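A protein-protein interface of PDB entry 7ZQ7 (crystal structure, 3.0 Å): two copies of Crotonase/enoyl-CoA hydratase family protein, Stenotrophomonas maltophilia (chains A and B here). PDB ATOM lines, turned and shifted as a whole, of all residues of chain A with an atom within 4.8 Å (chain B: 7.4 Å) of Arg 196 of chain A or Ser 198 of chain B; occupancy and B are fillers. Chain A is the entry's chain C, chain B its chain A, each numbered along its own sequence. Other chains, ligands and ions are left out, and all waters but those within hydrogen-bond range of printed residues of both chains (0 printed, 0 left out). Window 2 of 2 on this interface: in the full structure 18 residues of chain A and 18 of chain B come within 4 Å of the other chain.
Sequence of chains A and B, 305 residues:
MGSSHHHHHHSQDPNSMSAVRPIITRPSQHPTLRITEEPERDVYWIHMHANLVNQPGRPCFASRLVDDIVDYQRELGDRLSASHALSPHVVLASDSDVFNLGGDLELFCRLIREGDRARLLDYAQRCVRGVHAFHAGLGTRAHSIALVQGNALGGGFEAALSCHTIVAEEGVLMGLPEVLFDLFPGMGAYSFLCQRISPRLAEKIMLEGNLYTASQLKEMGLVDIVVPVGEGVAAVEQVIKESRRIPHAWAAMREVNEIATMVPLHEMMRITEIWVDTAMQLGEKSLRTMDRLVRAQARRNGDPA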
ATOM      1  N   LEU A 161     -37.525   4.173   6.187  1.00  0.00           N
ATOM      2  CA  LEU A 161     -36.815   4.760   7.330  1.00  0.00           C
ATOM      3  C   LEU A 161     -37.646   4.722   8.600  1.00  0.00           C
ATOM      4  O   LEU A 161     -37.090   4.778   9.703  1.00  0.00           O
ATOM      5  CB  LEU A 161     -36.425   6.203   7.041  1.00  0.00           C
ATOM      6  CG  LEU A 161     -35.260   6.460   6.105  1.00  0.00           C
ATOM      7  CD1 LEU A 161     -35.301   7.879   5.572  1.00  0.00           C
ATOM      8  CD2 LEU A 161     -34.003   6.219   6.898  1.00  0.00           C
ATOM      9  N   CYS A 163     -39.365   2.166   9.701  1.00  0.00           N
ATOM     10  CA  CYS A 163     -39.174   0.878  10.370  1.00  0.00           C
ATOM     11  C   CYS A 163     -37.910   0.870  11.220  1.00  0.00           C
ATOM     12  O   CYS A 163     -36.950   1.590  10.943  1.00  0.00           O
ATOM     13  CB  CYS A 163     -39.082  -0.261   9.355  1.00  0.00           C
ATOM     14  SG  CYS A 163     -40.611  -0.611   8.512  1.00  0.00           S
ATOM     15  N   HIS A 164     -37.898   0.006  12.248  1.00  0.00           N
ATOM     16  CA  HIS A 164     -36.737  -0.068  13.137  1.00  0.00           C
ATOM     17  C   HIS A 164     -35.527  -0.656  12.436  1.00  0.00           C
ATOM     18  O   HIS A 164     -34.387  -0.289  12.733  1.00  0.00           O
ATOM     19  CB  HIS A 164     -37.032  -0.902  14.372  1.00  0.00           C
ATOM     20  CG  HIS A 164     -38.268  -0.488  15.086  1.00  0.00           C
ATOM     21  ND1 HIS A 164     -39.518  -0.576  14.516  1.00  0.00           N
ATOM     22  CD2 HIS A 164     -38.451   0.032  16.320  1.00  0.00           C
ATOM     23  CE1 HIS A 164     -40.421  -0.138  15.374  1.00  0.00           C
ATOM     24  NE2 HIS A 164     -39.798   0.251  16.472  1.00  0.00           N
ATOM     25  N   ILE A 166     -33.896  -1.865   8.563  1.00  0.00           N
ATOM     26  CA  ILE A 166     -34.015  -1.731   7.116  1.00  0.00           C
ATOM     27  C   ILE A 166     -33.122  -2.800   6.497  1.00  0.00           C
ATOM     28  O   ILE A 166     -31.899  -2.806   6.707  1.00  0.00           O
ATOM     29  CB  ILE A 166     -33.650  -0.315   6.628  1.00  0.00           C
ATOM     30  CG1 ILE A 166     -34.823   0.645   6.866  1.00  0.00           C
ATOM     31  CG2 ILE A 166     -33.368  -0.293   5.146  1.00  0.00           C
ATOM     32  CD1 ILE A 166     -34.399   2.062   7.433  1.00  0.00           C
ATOM     33  N   PHE A 192     -37.453  10.716  10.852  1.00  0.00           N
ATOM     34  CA  PHE A 192     -36.716   9.456  10.976  1.00  0.00           C
ATOM     35  C   PHE A 192     -35.242   9.544  10.558  1.00  0.00           C
ATOM     36  O   PHE A 192     -34.442   8.711  11.010  1.00  0.00           O
ATOM     37  CB  PHE A 192     -37.426   8.344  10.180  1.00  0.00           C
ATOM     38  CG  PHE A 192     -38.918   8.271  10.434  1.00  0.00           C
ATOM     39  CD1 PHE A 192     -39.417   8.101  11.720  1.00  0.00           C
ATOM     40  CD2 PHE A 192     -39.822   8.379   9.391  1.00  0.00           C
ATOM     41  CE1 PHE A 192     -40.794   8.047  11.959  1.00  0.00           C
ATOM     42  CE2 PHE A 192     -41.207   8.331   9.626  1.00  0.00           C
ATOM     43  CZ  PHE A 192     -41.686   8.170  10.910  1.00  0.00           C
ATOM     44  N   LEU A 193     -34.858  10.529   9.728  1.00  0.00           N
ATOM     45  CA  LEU A 193     -33.445  10.722   9.380  1.00  0.00           C
ATOM     46  C   LEU A 193     -32.624  11.145  10.598  1.00  0.00           C
ATOM     47  O   LEU A 193     -31.557  10.580  10.874  1.00  0.00           O
ATOM     48  CB  LEU A 193     -33.311  11.774   8.275  1.00  0.00           C
ATOM     49  CG  LEU A 193     -33.598  11.368   6.835  1.00  0.00           C
ATOM     50  CD1 LEU A 193     -34.167  12.509   6.067  1.00  0.00           C
ATOM     51  CD2 LEU A 193     -32.334  10.873   6.158  1.00  0.00           C
ATOM     52  N   CYS A 194     -33.107  12.154  11.338  1.00  0.00           N
ATOM     53  CA  CYS A 194     -32.335  12.702  12.444  1.00  0.00           C
ATOM     54  C   CYS A 194     -32.086  11.677  13.527  1.00  0.00           C
ATOM     55  O   CYS A 194     -31.254  11.926  14.410  1.00  0.00           O
ATOM     56  CB  CYS A 194     -33.025  13.919  13.064  1.00  0.00           C
ATOM     57  SG  CYS A 194     -33.226  15.367  11.991  1.00  0.00           S
ATOM     58  N   GLN A 195     -32.806  10.552  13.494  1.00  0.00           N
ATOM     59  CA  GLN A 195     -32.530   9.436  14.383  1.00  0.00           C
ATOM     60  C   GLN A 195     -31.204   8.764  14.061  1.00  0.00           C
ATOM     61  O   GLN A 195     -30.605   8.127  14.938  1.00  0.00           O
ATOM     62  CB  GLN A 195     -33.650   8.414  14.275  1.00  0.00           C
ATOM     63  CG  GLN A 195     -35.005   8.906  14.687  1.00  0.00           C
ATOM     64  CD  GLN A 195     -35.357   8.432  16.077  1.00  0.00           C
ATOM     65  OE1 GLN A 195     -34.588   7.698  16.693  1.00  0.00           O
ATOM     66  NE2 GLN A 195     -36.541   8.806  16.561  1.00  0.00           N
ATOM     67  N   ARG A 196     -30.737   8.890  12.826  1.00  0.00           N
ATOM     68  CA  ARG A 196     -29.546   8.206  12.361  1.00  0.00           C
ATOM     69  C   ARG A 196     -28.363   9.135  12.159  1.00  0.00           C
ATOM     70  O   ARG A 196     -27.227   8.736  12.435  1.00  0.00           O
ATOM     71  CB  ARG A 196     -29.846   7.477  11.049  1.00  0.00           C
ATOM     72  CG  ARG A 196     -31.159   6.686  11.011  1.00  0.00           C
ATOM     73  CD  ARG A 196     -30.900   5.256  10.632  1.00  0.00           C
ATOM     74  NE  ARG A 196     -32.110   4.445  10.590  1.00  0.00           N
ATOM     75  CZ  ARG A 196     -32.116   3.122  10.742  1.00  0.00           C
ATOM     76  NH1 ARG A 196     -31.005   2.457  11.020  1.00  0.00           N
ATOM     77  NH2 ARG A 196     -33.271   2.458  10.660  1.00  0.00           N
ATOM     78  N   ILE A 197     -28.581  10.367  11.698  1.00  0.00           N
ATOM     79  CA  ILE A 197     -27.492  11.269  11.334  1.00  0.00           C
ATOM     80  C   ILE A 197     -27.797  12.692  11.809  1.00  0.00           C
ATOM     81  O   ILE A 197     -28.792  12.952  12.501  1.00  0.00           O
ATOM     82  CB  ILE A 197     -27.186  11.214   9.819  1.00  0.00           C
ATOM     83  CG1 ILE A 197     -28.448  11.072   8.984  1.00  0.00           C
ATOM     84  CG2 ILE A 197     -26.330  10.007   9.512  1.00  0.00           C
ATOM     85  CD1 ILE A 197     -29.239  12.269   8.799  1.00  0.00           C
ATOM     86  N   SER A 198     -26.885  13.622  11.500  1.00  0.00           N
ATOM     87  CA  SER A 198     -27.065  14.989  11.980  1.00  0.00           C
ATOM     88  C   SER A 198     -28.161  15.674  11.172  1.00  0.00           C
ATOM     89  O   SER A 198     -28.366  15.362   9.987  1.00  0.00           O
ATOM     90  CB  SER A 198     -25.773  15.811  11.902  1.00  0.00           C
ATOM     91  OG  SER A 198     -25.444  16.186  10.573  1.00  0.00           O
ATOM     92  N   GLY A 221     -25.204   4.861   7.539  1.00  0.00           N
ATOM     93  CA  GLY A 221     -26.015   4.548   8.694  1.00  0.00           C
ATOM     94  C   GLY A 221     -27.494   4.431   8.422  1.00  0.00           C
ATOM     95  O   GLY A 221     -28.266   4.190   9.361  1.00  0.00           O
ATOM     96  N   LEU A 222     -27.923   4.578   7.173  1.00  0.00           N
ATOM     97  CA  LEU A 222     -29.356   4.661   6.929  1.00  0.00           C
ATOM     98  C   LEU A 222     -29.957   3.278   6.687  1.00  0.00           C
ATOM     99  O   LEU A 222     -30.944   2.909   7.331  1.00  0.00           O
ATOM    100  CB  LEU A 222     -29.645   5.607   5.754  1.00  0.00           C
ATOM    101  CG  LEU A 222     -29.858   7.105   5.994  1.00  0.00           C
ATOM    102  CD1 LEU A 222     -28.921   7.662   7.033  1.00  0.00           C
ATOM    103  CD2 LEU A 222     -29.627   7.827   4.706  1.00  0.00           C
ATOM    104  N   ASP A 224     -29.789  -0.715   7.212  1.00  0.00           N
ATOM    105  CA  ASP A 224     -29.225  -1.533   8.280  1.00  0.00           C
ATOM    106  C   ASP A 224     -28.376  -2.673   7.730  1.00  0.00           C
ATOM    107  O   ASP A 224     -27.258  -2.914   8.207  1.00  0.00           O
ATOM    108  CB  ASP A 224     -30.344  -2.077   9.162  1.00  0.00           C
ATOM    109  CG  ASP A 224     -30.999  -0.999  10.002  1.00  0.00           C
ATOM    110  OD1 ASP A 224     -30.382  -0.544  10.992  1.00  0.00           O
ATOM    111  OD2 ASP A 224     -32.137  -0.599   9.670  1.00  0.00           O
ATOM    112  N   TYR B 190     -27.665   4.109  27.563  1.00  0.00           N
ATOM    113  CA  TYR B 190     -28.455   4.859  26.550  1.00  0.00           C
ATOM    114  C   TYR B 190     -28.120   6.351  26.650  1.00  0.00           C
ATOM    115  O   TYR B 190     -27.857   6.984  25.608  1.00  0.00           O
ATOM    116  CB  TYR B 190     -29.953   4.607  26.743  1.00  0.00           C
ATOM    117  CG  TYR B 190     -30.800   4.882  25.526  1.00  0.00           C
ATOM    118  CD1 TYR B 190     -30.261   4.823  24.252  1.00  0.00           C
ATOM    119  CD2 TYR B 190     -32.142   5.203  25.647  1.00  0.00           C
ATOM    120  CE1 TYR B 190     -31.032   5.074  23.129  1.00  0.00           C
ATOM    121  CE2 TYR B 190     -32.927   5.456  24.534  1.00  0.00           C
ATOM    122  CZ  TYR B 190     -32.371   5.392  23.271  1.00  0.00           C
ATOM    123  OH  TYR B 190     -33.137   5.642  22.169  1.00  0.00           O
ATOM    124  N   LEU B 193     -24.441   7.223  25.736  1.00  0.00           N
ATOM    125  CA  LEU B 193     -24.097   6.863  24.368  1.00  0.00           C
ATOM    126  C   LEU B 193     -24.541   7.938  23.389  1.00  0.00           C
ATOM    127  O   LEU B 193     -23.766   8.370  22.522  1.00  0.00           O
ATOM    128  CB  LEU B 193     -24.736   5.520  24.007  1.00  0.00           C
ATOM    129  CG  LEU B 193     -23.993   4.259  24.394  1.00  0.00           C
ATOM    130  CD1 LEU B 193     -24.851   3.090  23.944  1.00  0.00           C
ATOM    131  CD2 LEU B 193     -22.599   4.222  23.753  1.00  0.00           C
ATOM    132  N   CYS B 194     -25.800   8.369  23.520  1.00  0.00           N
ATOM    133  CA  CYS B 194     -26.397   9.372  22.656  1.00  0.00           C
ATOM    134  C   CYS B 194     -25.677  10.708  22.739  1.00  0.00           C
ATOM    135  O   CYS B 194     -26.004  11.613  21.966  1.00  0.00           O
ATOM    136  CB  CYS B 194     -27.863   9.556  23.028  1.00  0.00           C
ATOM    137  SG  CYS B 194     -28.938   8.201  22.578  1.00  0.00           S
ATOM    138  N   GLN B 195     -24.724  10.863  23.656  1.00  0.00           N
ATOM    139  CA  GLN B 195     -23.881  12.051  23.646  1.00  0.00           C
ATOM    140  C   GLN B 195     -22.763  11.972  22.622  1.00  0.00           C
ATOM    141  O   GLN B 195     -22.179  13.014  22.279  1.00  0.00           O
ATOM    142  CB  GLN B 195     -23.256  12.278  25.012  1.00  0.00           C
ATOM    143  CG  GLN B 195     -24.260  12.369  26.097  1.00  0.00           C
ATOM    144  CD  GLN B 195     -24.355  13.762  26.641  1.00  0.00           C
ATOM    145  OE1 GLN B 195     -23.387  14.527  26.586  1.00  0.00           O
ATOM    146  NE2 GLN B 195     -25.522  14.107  27.180  1.00  0.00           N
ATOM    147  N   ARG B 196     -22.430  10.767  22.150  1.00  0.00           N
ATOM    148  CA  ARG B 196     -21.327  10.599  21.223  1.00  0.00           C
ATOM    149  C   ARG B 196     -21.768  10.098  19.857  1.00  0.00           C
ATOM    150  O   ARG B 196     -21.063  10.340  18.859  1.00  0.00           O
ATOM    151  CB  ARG B 196     -20.287   9.627  21.817  1.00  0.00           C
ATOM    152  CG  ARG B 196     -19.512  10.143  23.042  1.00  0.00           C
ATOM    153  CD  ARG B 196     -19.257   9.005  24.011  1.00  0.00           C
ATOM    154  NE  ARG B 196     -18.627   9.387  25.269  1.00  0.00           N
ATOM    155  CZ  ARG B 196     -17.351   9.759  25.378  1.00  0.00           C
ATOM    156  NH1 ARG B 196     -16.541   9.776  24.319  1.00  0.00           N
ATOM    157  NH2 ARG B 196     -16.874  10.131  26.574  1.00  0.00           N
ATOM    158  N   ILE B 197     -22.919   9.436  19.777  1.00  0.00           N
ATOM    159  CA  ILE B 197     -23.345   8.747  18.569  1.00  0.00           C
ATOM    160  C   ILE B 197     -24.859   8.835  18.515  1.00  0.00           C
ATOM    161  O   ILE B 197     -25.521   9.045  19.542  1.00  0.00           O
ATOM    162  CB  ILE B 197     -22.867   7.262  18.550  1.00  0.00           C
ATOM    163  CG1 ILE B 197     -23.268   6.572  19.859  1.00  0.00           C
ATOM    164  CG2 ILE B 197     -21.352   7.135  18.254  1.00  0.00           C
ATOM    165  CD1 ILE B 197     -23.862   5.195  19.689  1.00  0.00           C
ATOM    166  N   SER B 198     -25.411   8.670  17.298  1.00  0.00           N
ATOM    167  CA  SER B 198     -26.851   8.803  17.070  1.00  0.00           C
ATOM    168  C   SER B 198     -27.631   7.789  17.901  1.00  0.00           C
ATOM    169  O   SER B 198     -27.142   6.690  18.166  1.00  0.00           O
ATOM    170  CB  SER B 198     -27.186   8.593  15.605  1.00  0.00           C
ATOM    171  OG  SER B 198     -26.892   7.261  15.194  1.00  0.00           O
ATOM    172  N   PRO B 199     -28.864   8.113  18.298  1.00  0.00           N
ATOM    173  CA  PRO B 199     -29.585   7.213  19.203  1.00  0.00           C
ATOM    174  C   PRO B 199     -29.949   5.879  18.552  1.00  0.00           C
ATOM    175  O   PRO B 199     -30.156   4.892  19.275  1.00  0.00           O
ATOM    176  CB  PRO B 199     -30.831   8.030  19.566  1.00  0.00           C
ATOM    177  CG  PRO B 199     -31.086   8.818  18.354  1.00  0.00           C
ATOM    178  CD  PRO B 199     -29.725   9.225  17.861  1.00  0.00           C
ATOM    179  N   ARG B 200     -30.029   5.829  17.210  1.00  0.00           N
ATOM    180  CA  ARG B 200     -30.258   4.569  16.510  1.00  0.00           C
ATOM    181  C   ARG B 200     -29.053   3.658  16.656  1.00  0.00           C
ATOM    182  O   ARG B 200     -29.194   2.481  17.012  1.00  0.00           O
ATOM    183  CB  ARG B 200     -30.558   4.821  15.028  1.00  0.00           C
ATOM    184  CG  ARG B 200     -31.210   3.668  14.243  1.00  0.00           C
ATOM    185  CD  ARG B 200     -32.252   2.916  15.016  1.00  0.00           C
ATOM    186  NE  ARG B 200     -32.285   1.538  14.539  1.00  0.00           N
ATOM    187  CZ  ARG B 200     -32.967   0.542  15.099  1.00  0.00           C
ATOM    188  NH1 ARG B 200     -33.811   0.759  16.104  1.00  0.00           N
ATOM    189  NH2 ARG B 200     -32.826  -0.697  14.615  1.00  0.00           N
ATOM    190  N   LEU B 201     -27.854   4.184  16.384  1.00  0.00           N
ATOM    191  CA  LEU B 201     -26.632   3.431  16.669  1.00  0.00           C
ATOM    192  C   LEU B 201     -26.507   3.087  18.155  1.00  0.00           C
ATOM    193  O   LEU B 201     -25.969   2.020  18.512  1.00  0.00           O
ATOM    194  CB  LEU B 201     -25.400   4.216  16.215  1.00  0.00           C
ATOM    195  CG  LEU B 201     -24.142   3.354  16.249  1.00  0.00           C
ATOM    196  CD1 LEU B 201     -24.371   2.083  15.426  1.00  0.00           C
ATOM    197  CD2 LEU B 201     -22.917   4.104  15.792  1.00  0.00           C
ATOM    198  N   ALA B 202     -26.978   3.971  19.042  1.00  0.00           N
ATOM    199  CA  ALA B 202     -26.989   3.608  20.455  1.00  0.00           C
ATOM    200  C   ALA B 202     -27.792   2.335  20.678  1.00  0.00           C
ATOM    201  O   ALA B 202     -27.411   1.502  21.499  1.00  0.00           O
ATOM    202  CB  ALA B 202     -27.537   4.748  21.308  1.00  0.00           C
ATOM    203  N   GLU B 203     -28.879   2.148  19.914  1.00  0.00           N
ATOM    204  CA  GLU B 203     -29.746   0.989  20.115  1.00  0.00           C
ATOM    205  C   GLU B 203     -29.051  -0.291  19.648  1.00  0.00           C
ATOM    206  O   GLU B 203     -28.946  -1.266  20.410  1.00  0.00           O
ATOM    207  CB  GLU B 203     -31.082   1.172  19.378  1.00  0.00           C
ATOM    208  CG  GLU B 203     -32.317   0.645  20.155  1.00  0.00           C
ATOM    209  CD  GLU B 203     -33.395  -0.049  19.275  1.00  0.00           C
ATOM    210  OE1 GLU B 203     -33.099  -0.637  18.181  1.00  0.00           O
ATOM    211  OE2 GLU B 203     -34.557  -0.031  19.729  1.00  0.00           O
ATOM    212  N   LYS B 204     -28.567  -0.301  18.400  1.00  0.00           N
ATOM    213  CA  LYS B 204     -27.752  -1.392  17.890  1.00  0.00           C
ATOM    214  C   LYS B 204     -26.637  -1.957  18.766  1.00  0.00           C
ATOM    215  O   LYS B 204     -26.580  -3.174  18.970  1.00  0.00           O
ATOM    216  CB  LYS B 204     -27.010  -0.959  16.626  1.00  0.00           C
ATOM    217  CG  LYS B 204     -27.878  -0.915  15.372  1.00  0.00           C
ATOM    218  CD  LYS B 204     -27.221  -1.620  14.178  1.00  0.00           C
ATOM    219  CE  LYS B 204     -27.447  -0.807  12.897  1.00  0.00           C
ATOM    220  NZ  LYS B 204     -28.897  -0.490  12.721  1.00  0.00           N
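Ser 198 of chain B touches Gln 195 of chain A.
Gln 195 of chain A touches Pro 199 of chain B (O to CD, 3.2 Å).
Arg 196 of chain A touches Arg 200 of chain B.
Gln 195 of chain A touches Ser 198 of chain B, but with the chains exchanged Ser 198 of chain A does not touch Gln 195 of chain B (11.3 Å).
Arg 196 of chain A touches Ser 198 of chain B, but with the chains exchanged Ser 198 of chain A does not touch Arg 196 of chain B (9.9 Å).
Of the 7 pairs that touch across the chains among the printed residues, none has its exchanged pair printed and touching as well.
Of the 13 printed residues of chain B, 4 touch a printed residue of chain A.
Of the 14 printed residues of chain A, 4 touch a printed residue of chain B.
Printed residues of chain A that touch a printed residue of chain B: His 164, Gln 195, Arg 196 and Asp 224.
Among the printed residues, Asp or Glu carboxylates within 4 Å of a Lys or Arg side-chain nitrogen of the other chain: Asp 224 of chain A with Lys 204 of chain B (2.3 Å).
Printed residues of chain B within 4 Å of Arg 196 of chain A: Ser 198 (3.1 Å) and Arg 200 (3.4 Å).
Of chain A, only Gln 195 and Arg 196 come within 4 Å of Ser 198 of chain B.
Of the printed residues of chain A, Pro 199 of chain B touches Gln 195.
Printed residues of chain B within 4 Å of Asp 224 of chain A: Lys 204 (2.3 Å).
Of the printed residues of chain B, His 164 of chain A touches Arg 200 (2.5 Å).
The nearest printed residue of chain B that does not touch Arg 196 of chain A is Lys 204 of chain B (4.003 Å).
The nearest residue of chain A that does not touch Ser 198 of chain B is Ile 197 of chain A (4.5 Å).
The nearest printed residue of chain B that does not touch Asp 224 of chain A is Arg 200 of chain B (4.4 Å).
The backbone NH (N) of Leu 201 of chain B lies within hydrogen-bond range of the side-chain hydroxyl (OG) of Ser 198 of chain B (3.4 Å).
OE1 of Glu 203 of chain B lies within salt-bridge range of NH1 of Arg 200 of chain B (2.6 Å).
The backbone NH (N) of Ile 166 of chain A sits at hydrogen-bond distance from the side-chain carboxylate (OD2) of Asp 224 of chain A (2.4 Å).
OD1 of Asp 224 of chain A lies within salt-bridge range of NH1 of Arg 196 of chain A, at 3.1 Å.
The backbone carbonyl oxygen (O) of Arg 196 of chain A is in hydrogen-bond range of the side-chain hydroxyl (OG) of Ser 198 of chain B (3.1 Å).
NH2 of Arg 200 of chain B lies within hydrogen-bond range of O of His 164 of chain A (2.5 Å).
N of Arg 200 of chain B lies within hydrogen-bond range of O of Gln 195 of chain A (3.3 Å).
OD1 of Asp 224 of chain A sits close to NZ of Lys 204 of chain B.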
